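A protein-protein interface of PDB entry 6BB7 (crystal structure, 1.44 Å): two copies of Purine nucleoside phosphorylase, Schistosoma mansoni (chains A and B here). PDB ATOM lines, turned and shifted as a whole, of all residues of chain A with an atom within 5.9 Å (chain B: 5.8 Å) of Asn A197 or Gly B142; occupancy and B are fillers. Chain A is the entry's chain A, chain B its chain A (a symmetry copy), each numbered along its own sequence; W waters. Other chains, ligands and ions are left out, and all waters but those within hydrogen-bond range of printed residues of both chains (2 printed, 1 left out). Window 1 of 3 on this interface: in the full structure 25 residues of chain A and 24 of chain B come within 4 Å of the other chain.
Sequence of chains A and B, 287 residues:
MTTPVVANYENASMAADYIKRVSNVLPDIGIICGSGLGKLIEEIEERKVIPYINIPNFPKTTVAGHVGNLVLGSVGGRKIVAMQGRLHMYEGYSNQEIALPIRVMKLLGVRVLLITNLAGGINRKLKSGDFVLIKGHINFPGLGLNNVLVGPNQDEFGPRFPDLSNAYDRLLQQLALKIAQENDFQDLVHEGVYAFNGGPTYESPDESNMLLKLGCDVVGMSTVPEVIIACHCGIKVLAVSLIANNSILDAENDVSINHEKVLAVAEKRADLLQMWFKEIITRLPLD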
ATOM      1  N   ILE A 138     -12.281 -15.322 -10.868  1.00  0.00           N
ATOM      2  CA  ILE A 138     -11.091 -14.654 -10.337  1.00  0.00           C
ATOM      3  C   ILE A 138     -10.333 -14.059 -11.534  1.00  0.00           C
ATOM      4  O   ILE A 138      -9.794 -14.785 -12.383  1.00  0.00           O
ATOM      5  CB  ILE A 138     -10.208 -15.589  -9.502  1.00  0.00           C
ATOM      6  CG1 ILE A 138     -10.970 -16.059  -8.245  1.00  0.00           C
ATOM      7  CG2 ILE A 138      -8.891 -14.896  -9.108  1.00  0.00           C
ATOM      8  CD1 ILE A 138     -10.284 -17.168  -7.498  1.00  0.00           C
ATOM      9  N   PHE A 140      -7.451 -12.310 -12.860  1.00  0.00           N
ATOM     10  CA  PHE A 140      -6.057 -11.900 -12.649  1.00  0.00           C
ATOM     11  C   PHE A 140      -5.701 -10.654 -13.456  1.00  0.00           C
ATOM     12  O   PHE A 140      -5.048  -9.747 -12.882  1.00  0.00           O
ATOM     13  CB  PHE A 140      -5.090 -13.080 -12.881  1.00  0.00           C
ATOM     14  CG  PHE A 140      -5.173 -14.133 -11.800  1.00  0.00           C
ATOM     15  CD1 PHE A 140      -4.650 -13.901 -10.540  1.00  0.00           C
ATOM     16  CD2 PHE A 140      -5.792 -15.346 -12.049  1.00  0.00           C
ATOM     17  CE1 PHE A 140      -4.744 -14.877  -9.533  1.00  0.00           C
ATOM     18  CE2 PHE A 140      -5.890 -16.307 -11.040  1.00  0.00           C
ATOM     19  CZ  PHE A 140      -5.368 -16.077  -9.803  1.00  0.00           C
ATOM     20  N   PRO A 141      -6.079 -10.532 -14.739  1.00  0.00           N
ATOM     21  CA  PRO A 141      -5.814  -9.255 -15.432  1.00  0.00           C
ATOM     22  C   PRO A 141      -6.437  -8.050 -14.723  1.00  0.00           C
ATOM     23  O   PRO A 141      -5.791  -6.992 -14.625  1.00  0.00           O
ATOM     24  CB  PRO A 141      -6.353  -9.489 -16.853  1.00  0.00           C
ATOM     25  CG  PRO A 141      -6.162 -11.005 -17.041  1.00  0.00           C
ATOM     26  CD  PRO A 141      -6.591 -11.551 -15.679  1.00  0.00           C
ATOM     27  N   TYR A 194     -14.339 -19.684 -12.206  1.00  0.00           N
ATOM     28  CA  TYR A 194     -13.454 -19.602 -13.375  1.00  0.00           C
ATOM     29  C   TYR A 194     -12.327 -18.603 -13.131  1.00  0.00           C
ATOM     30  O   TYR A 194     -12.592 -17.420 -12.865  1.00  0.00           O
ATOM     31  CB  TYR A 194     -14.270 -19.163 -14.586  1.00  0.00           C
ATOM     32  CG  TYR A 194     -13.552 -19.019 -15.915  1.00  0.00           C
ATOM     33  CD1 TYR A 194     -13.594 -20.046 -16.866  1.00  0.00           C
ATOM     34  CD2 TYR A 194     -12.872 -17.837 -16.265  1.00  0.00           C
ATOM     35  CE1 TYR A 194     -12.972 -19.917 -18.105  1.00  0.00           C
ATOM     36  CE2 TYR A 194     -12.253 -17.694 -17.500  1.00  0.00           C
ATOM     37  CZ  TYR A 194     -12.292 -18.732 -18.421  1.00  0.00           C
ATOM     38  OH  TYR A 194     -11.724 -18.633 -19.660  1.00  0.00           O
ATOM     39  N   ALA A 195     -11.077 -19.068 -13.242  1.00  0.00           N
ATOM     40  CA  ALA A 195      -9.901 -18.189 -13.238  1.00  0.00           C
ATOM     41  C   ALA A 195      -9.539 -17.766 -14.661  1.00  0.00           C
ATOM     42  O   ALA A 195      -9.395 -18.613 -15.555  1.00  0.00           O
ATOM     43  CB  ALA A 195      -8.698 -18.889 -12.606  1.00  0.00           C
ATOM     44  N   PHE A 196      -9.361 -16.449 -14.859  1.00  0.00           N
ATOM     45  CA  PHE A 196      -8.932 -15.882 -16.140  1.00  0.00           C
ATOM     46  C   PHE A 196      -7.397 -15.779 -16.163  1.00  0.00           C
ATOM     47  O   PHE A 196      -6.806 -14.968 -15.436  1.00  0.00           O
ATOM     48  CB  PHE A 196      -9.604 -14.517 -16.331  1.00  0.00           C
ATOM     49  CG  PHE A 196      -9.283 -13.795 -17.656  1.00  0.00           C
ATOM     50  CD1 PHE A 196      -8.819 -14.458 -18.800  1.00  0.00           C
ATOM     51  CD2 PHE A 196      -9.460 -12.407 -17.721  1.00  0.00           C
ATOM     52  CE1 PHE A 196      -8.528 -13.758 -19.968  1.00  0.00           C
ATOM     53  CE2 PHE A 196      -9.172 -11.714 -18.889  1.00  0.00           C
ATOM     54  CZ  PHE A 196      -8.701 -12.374 -20.010  1.00  0.00           C
ATOM     55  N   ASN A 197      -6.762 -16.654 -16.959  1.00  0.00           N
ATOM     56  CA  ASN A 197      -5.340 -16.602 -17.341  1.00  0.00           C
ATOM     57  C   ASN A 197      -5.247 -15.850 -18.670  1.00  0.00           C
ATOM     58  O   ASN A 197      -5.760 -16.311 -19.687  1.00  0.00           O
ATOM     59  CB  ASN A 197      -4.788 -18.029 -17.510  1.00  0.00           C
ATOM     60  CG  ASN A 197      -3.451 -18.092 -18.252  1.00  0.00           C
ATOM     61  OD1 ASN A 197      -2.623 -17.176 -18.157  1.00  0.00           O
ATOM     62  ND2 ASN A 197      -3.231 -19.194 -18.998  1.00  0.00           N
ATOM     63  N   GLY A 198      -4.586 -14.690 -18.673  1.00  0.00           N
ATOM     64  CA  GLY A 198      -4.481 -13.924 -19.909  1.00  0.00           C
ATOM     65  C   GLY A 198      -3.978 -14.729 -21.102  1.00  0.00           C
ATOM     66  O   GLY A 198      -4.417 -14.512 -22.239  1.00  0.00           O
ATOM     67  N   GLY A 199      -3.018 -15.630 -20.892  1.00  0.00           N
ATOM     68  CA  GLY A 199      -2.545 -16.490 -21.984  1.00  0.00           C
ATOM     69  C   GLY A 199      -1.471 -15.826 -22.863  1.00  0.00           C
ATOM     70  O   GLY A 199      -1.001 -14.712 -22.549  1.00  0.00           O
ATOM     71  N   PRO A 200      -1.064 -16.460 -23.976  1.00  0.00           N
ATOM     72  CA  PRO A 200      -1.635 -17.663 -24.608  1.00  0.00           C
ATOM     73  C   PRO A 200      -0.984 -18.993 -24.190  1.00  0.00           C
ATOM     74  O   PRO A 200      -1.372 -20.037 -24.718  1.00  0.00           O
ATOM     75  CB  PRO A 200      -1.366 -17.396 -26.093  1.00  0.00           C
ATOM     76  CG  PRO A 200      -0.012 -16.665 -26.084  1.00  0.00           C
ATOM     77  CD  PRO A 200      -0.071 -15.800 -24.845  1.00  0.00           C
ATOM     78  N   THR A 201       0.023 -18.983 -23.308  1.00  0.00           N
ATOM     79  CA  THR A 201       0.557 -20.246 -22.796  1.00  0.00           C
ATOM     80  C   THR A 201      -0.457 -20.887 -21.844  1.00  0.00           C
ATOM     81  O   THR A 201      -1.069 -20.206 -21.020  1.00  0.00           O
ATOM     82  CB  THR A 201       1.908 -20.037 -22.070  1.00  0.00           C
ATOM     83  OG1 THR A 201       1.774 -19.063 -21.042  1.00  0.00           O
ATOM     84  CG2 THR A 201       3.016 -19.535 -23.031  1.00  0.00           C
ATOM     85  N   TYR A 202      -0.610 -22.216 -21.955  1.00  0.00           N
ATOM     86  CA  TYR A 202      -1.427 -22.946 -20.982  1.00  0.00           C
ATOM     87  C   TYR A 202      -0.838 -22.732 -19.584  1.00  0.00           C
ATOM     88  O   TYR A 202       0.370 -22.527 -19.422  1.00  0.00           O
ATOM     89  CB  TYR A 202      -1.479 -24.444 -21.327  1.00  0.00           C
ATOM     90  CG  TYR A 202      -2.184 -24.768 -22.651  1.00  0.00           C
ATOM     91  CD1 TYR A 202      -3.556 -24.545 -22.812  1.00  0.00           C
ATOM     92  CD2 TYR A 202      -1.469 -25.250 -23.730  1.00  0.00           C
ATOM     93  CE1 TYR A 202      -4.200 -24.854 -24.026  1.00  0.00           C
ATOM     94  CE2 TYR A 202      -2.111 -25.564 -24.944  1.00  0.00           C
ATOM     95  CZ  TYR A 202      -3.472 -25.318 -25.079  1.00  0.00           C
ATOM     96  OH  TYR A 202      -4.129 -25.603 -26.277  1.00  0.00           O
ATOM     97  N   GLU A 203      -1.708 -22.746 -18.574  1.00  0.00           N
ATOM     98  CA  GLU A 203      -1.249 -22.738 -17.184  1.00  0.00           C
ATOM     99  C   GLU A 203      -0.132 -23.762 -16.969  1.00  0.00           C
ATOM    100  O   GLU A 203      -0.243 -24.922 -17.372  1.00  0.00           O
ATOM    101  CB  GLU A 203      -2.440 -23.032 -16.242  1.00  0.00           C
ATOM    102  CG  GLU A 203      -3.138 -24.446 -16.325  1.00  0.00           C
ATOM    103  CD  GLU A 203      -4.203 -24.602 -17.409  1.00  0.00           C
ATOM    104  OE1 GLU A 203      -4.372 -23.718 -18.270  1.00  0.00           O
ATOM    105  OE2 GLU A 203      -4.885 -25.670 -17.410  1.00  0.00           O
ATOM    106  N   GLU A 207       1.627 -23.160 -11.730  1.00  0.00           N
ATOM    107  CA  GLU A 207       0.469 -22.276 -11.708  1.00  0.00           C
ATOM    108  C   GLU A 207      -0.820 -23.046 -11.381  1.00  0.00           C
ATOM    109  O   GLU A 207      -1.668 -22.552 -10.630  1.00  0.00           O
ATOM    110  CB  GLU A 207       0.349 -21.507 -13.038  1.00  0.00           C
ATOM    111  CG  GLU A 207       1.495 -20.478 -13.237  1.00  0.00           C
ATOM    112  CD  GLU A 207       1.753 -20.086 -14.685  1.00  0.00           C
ATOM    113  OE1 GLU A 207       1.032 -20.522 -15.619  1.00  0.00           O
ATOM    114  OE2 GLU A 207       2.711 -19.299 -14.893  1.00  0.00           O
ATOM    115  N   VAL A 219      -9.807 -23.019 -15.281  1.00  0.00           N
ATOM    116  CA  VAL A 219      -8.960 -21.914 -15.751  1.00  0.00           C
ATOM    117  C   VAL A 219      -9.033 -21.824 -17.281  1.00  0.00           C
ATOM    118  O   VAL A 219      -8.973 -22.835 -17.981  1.00  0.00           O
ATOM    119  CB  VAL A 219      -7.499 -22.063 -15.241  1.00  0.00           C
ATOM    120  CG1 VAL A 219      -6.866 -23.367 -15.678  1.00  0.00           C
ATOM    121  CG2 VAL A 219      -6.625 -20.900 -15.687  1.00  0.00           C
ATOM    122  N   GLY A 220      -9.155 -20.601 -17.805  1.00  0.00           N
ATOM    123  CA  GLY A 220      -9.099 -20.401 -19.247  1.00  0.00           C
ATOM    124  C   GLY A 220      -8.700 -18.985 -19.617  1.00  0.00           C
ATOM    125  O   GLY A 220      -8.456 -18.143 -18.741  1.00  0.00           O
ATOM    126  N   MET A 221      -8.703 -18.716 -20.937  1.00  0.00           N
ATOM    127  CA  MET A 221      -8.105 -17.512 -21.522  1.00  0.00           C
ATOM    128  C   MET A 221      -9.125 -16.561 -22.148  1.00  0.00           C
ATOM    129  O   MET A 221      -8.743 -15.703 -22.952  1.00  0.00           O
ATOM    130  CB  MET A 221      -7.043 -17.877 -22.571  1.00  0.00           C
ATOM    131  CG  MET A 221      -5.966 -18.828 -22.136  1.00  0.00           C
ATOM    132  SD  MET A 221      -4.930 -19.319 -23.558  1.00  0.00           S
ATOM    133  CE  MET A 221      -4.085 -20.714 -22.826  1.00  0.00           C
ATOM    134  N   SER A 222     -10.408 -16.700 -21.834  1.00  0.00           N
ATOM    135  CA  SER A 222     -11.450 -15.907 -22.495  1.00  0.00           C
ATOM    136  C   SER A 222     -12.568 -15.597 -21.499  1.00  0.00           C
ATOM    137  O   SER A 222     -12.422 -15.780 -20.282  1.00  0.00           O
ATOM    138  CB  SER A 222     -11.996 -16.648 -23.732  1.00  0.00           C
ATOM    139  OG  SER A 222     -12.697 -17.807 -23.360  1.00  0.00           O
ATOM    140  N   ASN B 139       4.080 -17.315 -13.235  1.00  0.00           N
ATOM    141  CA  ASN B 139       4.268 -16.149 -14.122  1.00  0.00           C
ATOM    142  C   ASN B 139       3.144 -15.139 -13.873  1.00  0.00           C
ATOM    143  O   ASN B 139       2.123 -15.129 -14.570  1.00  0.00           O
ATOM    144  CB  ASN B 139       4.260 -16.674 -15.570  1.00  0.00           C
ATOM    145  CG  ASN B 139       4.471 -15.610 -16.627  1.00  0.00           C
ATOM    146  OD1 ASN B 139       4.773 -14.440 -16.361  1.00  0.00           O
ATOM    147  ND2 ASN B 139       4.295 -16.040 -17.886  1.00  0.00           N
ATOM    148  N   PHE B 140       3.326 -14.280 -12.853  1.00  0.00           N
ATOM    149  CA  PHE B 140       2.288 -13.292 -12.533  1.00  0.00           C
ATOM    150  C   PHE B 140       1.984 -12.380 -13.718  1.00  0.00           C
ATOM    151  O   PHE B 140       0.780 -12.140 -13.984  1.00  0.00           O
ATOM    152  CB  PHE B 140       2.632 -12.525 -11.239  1.00  0.00           C
ATOM    153  CG  PHE B 140       2.512 -13.377  -9.997  1.00  0.00           C
ATOM    154  CD1 PHE B 140       1.271 -13.739  -9.500  1.00  0.00           C
ATOM    155  CD2 PHE B 140       3.645 -13.828  -9.343  1.00  0.00           C
ATOM    156  CE1 PHE B 140       1.164 -14.545  -8.354  1.00  0.00           C
ATOM    157  CE2 PHE B 140       3.531 -14.637  -8.210  1.00  0.00           C
ATOM    158  CZ  PHE B 140       2.308 -14.985  -7.721  1.00  0.00           C
ATOM    159  N   PRO B 141       2.976 -11.856 -14.458  1.00  0.00           N
ATOM    160  CA  PRO B 141       2.620 -11.081 -15.664  1.00  0.00           C
ATOM    161  C   PRO B 141       1.772 -11.879 -16.656  1.00  0.00           C
ATOM    162  O   PRO B 141       0.812 -11.330 -17.227  1.00  0.00           O
ATOM    163  CB  PRO B 141       3.979 -10.632 -16.226  1.00  0.00           C
ATOM    164  CG  PRO B 141       4.850 -10.527 -14.961  1.00  0.00           C
ATOM    165  CD  PRO B 141       4.425 -11.770 -14.178  1.00  0.00           C
ATOM    166  N   GLY B 142       2.094 -13.156 -16.896  1.00  0.00           N
ATOM    167  CA  GLY B 142       1.320 -13.964 -17.841  1.00  0.00           C
ATOM    168  C   GLY B 142      -0.131 -14.166 -17.417  1.00  0.00           C
ATOM    169  O   GLY B 142      -1.059 -14.038 -18.231  1.00  0.00           O
ATOM    170  N   LEU B 143      -0.371 -14.485 -16.135  1.00  0.00           N
ATOM    171  CA  LEU B 143      -1.747 -14.599 -15.660  1.00  0.00           C
ATOM    172  C   LEU B 143      -2.490 -13.283 -15.871  1.00  0.00           C
ATOM    173  O   LEU B 143      -3.692 -13.284 -16.170  1.00  0.00           O
ATOM    174  CB  LEU B 143      -1.796 -15.030 -14.184  1.00  0.00           C
ATOM    175  CG  LEU B 143      -1.267 -16.458 -13.887  1.00  0.00           C
ATOM    176  CD1 LEU B 143      -1.164 -16.649 -12.386  1.00  0.00           C
ATOM    177  CD2 LEU B 143      -2.172 -17.545 -14.465  1.00  0.00           C
ATOM    178  N   GLY B 144      -1.787 -12.146 -15.711  1.00  0.00           N
ATOM    179  CA  GLY B 144      -2.372 -10.802 -15.763  1.00  0.00           C
ATOM    180  C   GLY B 144      -2.398 -10.058 -17.088  1.00  0.00           C
ATOM    181  O   GLY B 144      -2.571  -8.819 -17.100  1.00  0.00           O
ATOM    182  N   LEU B 145      -2.314 -10.775 -18.218  1.00  0.00           N
ATOM    183  CA  LEU B 145      -2.397 -10.239 -19.590  1.00  0.00           C
ATOM    184  C   LEU B 145      -1.132  -9.526 -20.074  1.00  0.00           C
ATOM    185  O   LEU B 145      -1.172  -8.815 -21.104  1.00  0.00           O
ATOM    186  CB  LEU B 145      -3.676  -9.416 -19.877  1.00  0.00           C
ATOM    187  CG  LEU B 145      -4.810 -10.172 -20.587  1.00  0.00           C
ATOM    188  CD1 LEU B 145      -6.029  -9.298 -20.683  1.00  0.00           C
ATOM    189  CD2 LEU B 145      -4.403 -10.677 -21.996  1.00  0.00           C
ATOM    190  N   ASN B 146       0.016  -9.730 -19.398  1.00  0.00           N
ATOM    191  CA  ASN B 146       1.325  -9.237 -19.829  1.00  0.00           C
ATOM    192  C   ASN B 146       2.309 -10.376 -20.175  1.00  0.00           C
ATOM    193  O   ASN B 146       3.522 -10.203 -20.091  1.00  0.00           O
ATOM    194  CB  ASN B 146       1.917  -8.250 -18.813  1.00  0.00           C
ATOM    195  CG  ASN B 146       1.271  -6.872 -18.862  1.00  0.00           C
ATOM    196  OD1 ASN B 146       0.733  -6.456 -19.885  1.00  0.00           O
ATOM    197  ND2 ASN B 146       1.302  -6.156 -17.731  1.00  0.00           N
ATOM    198  N   ASN B 147       1.813 -11.554 -20.574  1.00  0.00           N
ATOM    199  CA  ASN B 147       2.708 -12.604 -21.107  1.00  0.00           C
ATOM    200  C   ASN B 147       3.532 -12.070 -22.284  1.00  0.00           C
ATOM    201  O   ASN B 147       3.023 -11.304 -23.105  1.00  0.00           O
ATOM    202  CB  ASN B 147       1.831 -13.791 -21.574  1.00  0.00           C
ATOM    203  CG  ASN B 147       2.588 -15.119 -21.763  1.00  0.00           C
ATOM    204  OD1 ASN B 147       3.471 -15.241 -22.626  1.00  0.00           O
ATOM    205  ND2 ASN B 147       2.192 -16.147 -20.994  1.00  0.00           N
ATOM    206  N   PHE B 196       7.885 -14.940 -10.968  1.00  0.00           N
ATOM    207  CA  PHE B 196       8.243 -13.746 -11.738  1.00  0.00           C
ATOM    208  C   PHE B 196       7.467 -12.536 -11.192  1.00  0.00           C
ATOM    209  O   PHE B 196       6.240 -12.449 -11.346  1.00  0.00           O
ATOM    210  CB  PHE B 196       7.946 -14.001 -13.220  1.00  0.00           C
ATOM    211  CG  PHE B 196       8.301 -12.846 -14.180  1.00  0.00           C
ATOM    212  CD1 PHE B 196       9.225 -11.842 -13.865  1.00  0.00           C
ATOM    213  CD2 PHE B 196       7.667 -12.796 -15.428  1.00  0.00           C
ATOM    214  CE1 PHE B 196       9.500 -10.811 -14.760  1.00  0.00           C
ATOM    215  CE2 PHE B 196       7.947 -11.769 -16.318  1.00  0.00           C
ATOM    216  CZ  PHE B 196       8.850 -10.772 -15.995  1.00  0.00           C
HETATM  217  O   HOH W   1       0.164 -17.020 -18.950  1.00  0.00           O
HETATM  218  O   HOH W   2       3.635 -19.097 -17.580  1.00  0.00           O
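Printed residues of chain B within 4 Å of Pro A141: Leu B143, Gly B144 and Leu B145.
Of the printed residues of chain B, Gly A198 touches Gly B142, Leu B143 and Leu B145.
Gly A220 touches none of the printed residues of chain B.
Of the printed residues of chain A, Asn B139 touches Glu A207 (2.9 Å).
Gly B142 touches three residues of chain A.
Of the printed residues of chain A, Gly B144 touches Pro A141.
Phe B196 touches none of the printed residues of chain A.
The nearest printed residue of chain A that does not touch Gly B142 is Thr A201 (6.0 Å).
The nearest printed residue of chain B that does not touch Phe A140 is Gly B144 (4.1 Å).
The backbone NH of Gly B142 is in hydrogen-bond range of the side-chain amide oxygen of Asn B139, at 3.0 Å.
The backbone NH of Phe A196 is in hydrogen-bond range of the backbone carbonyl oxygen of Ile A138, at 3.0 Å.
N of Asn A197 sits at hydrogen-bond distance from O of Gly A220, 2.9 Å away.
OD1 of Asn A197 sits close to N of Gly A199 (3.2 Å).
O of Thr A201 is in hydrogen-bond range of ND2 of Asn A197.
3 positions are printed for both chains.
Water W2 lies within hydrogen-bond range of the side-chain carboxylate (OE2) of Glu A207 (2.8 Å) and the side-chain amide nitrogen (ND2) of Asn B139 (3.1 Å).
Water W1 lies within hydrogen-bond range of the side-chain amide oxygen of Asn A197 (2.9 Å), the side-chain amide nitrogen of Asn B147 (3.0 Å), the backbone carbonyl oxygen of Gly B142 (3.3 Å) and the side-chain hydroxyl of Thr A201 (3.3 Å).
Printed residues of chain A that touch a printed residue of chain B: Phe A140, Pro A141, Phe A196, Asn A197, Gly A198, Gly A199, Thr A201 and Glu A207.
Of the 10 printed residues of chain B, 6 touch a printed residue of chain A.
Printed residues of chain B that touch a printed residue of chain A: Asn B139, Gly B142, Leu B143, Gly B144, Leu B145 and Asn B147.
Among the printed residues, 14 pairs touch across the chains.
Among the printed residues, no Asp or Glu carboxylate lies within 4 Å of a Lys or Arg side-chain nitrogen of the other chain.
OG1 of Thr A201 is in hydrogen-bond range of ND2 of Asn B147, at 2.9 Å.
The side-chain carboxylate (OE2) of Glu A207 sits at hydrogen-bond distance from the backbone NH (N) of Asn B139 (2.9 Å).
The backbone carbonyl oxygen (O) of Leu B143 sits at hydrogen-bond distance from the backbone NH (N) of Gly A198 (3.0 Å).
Among the printed residues, pairs that only touch across the chains: Phe A140 with Leu B143, Pro A141 with Leu B143, Pro A141 with Gly B144, Pro A141 with Leu B145, Phe A196 with Leu B143, Asn A197 with Gly B142, Asn A197 with Leu B143, Gly A198 with Gly B142, Gly A198 with Leu B145, Gly A199 with Gly B142 and Gly A199 with Asn B147.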
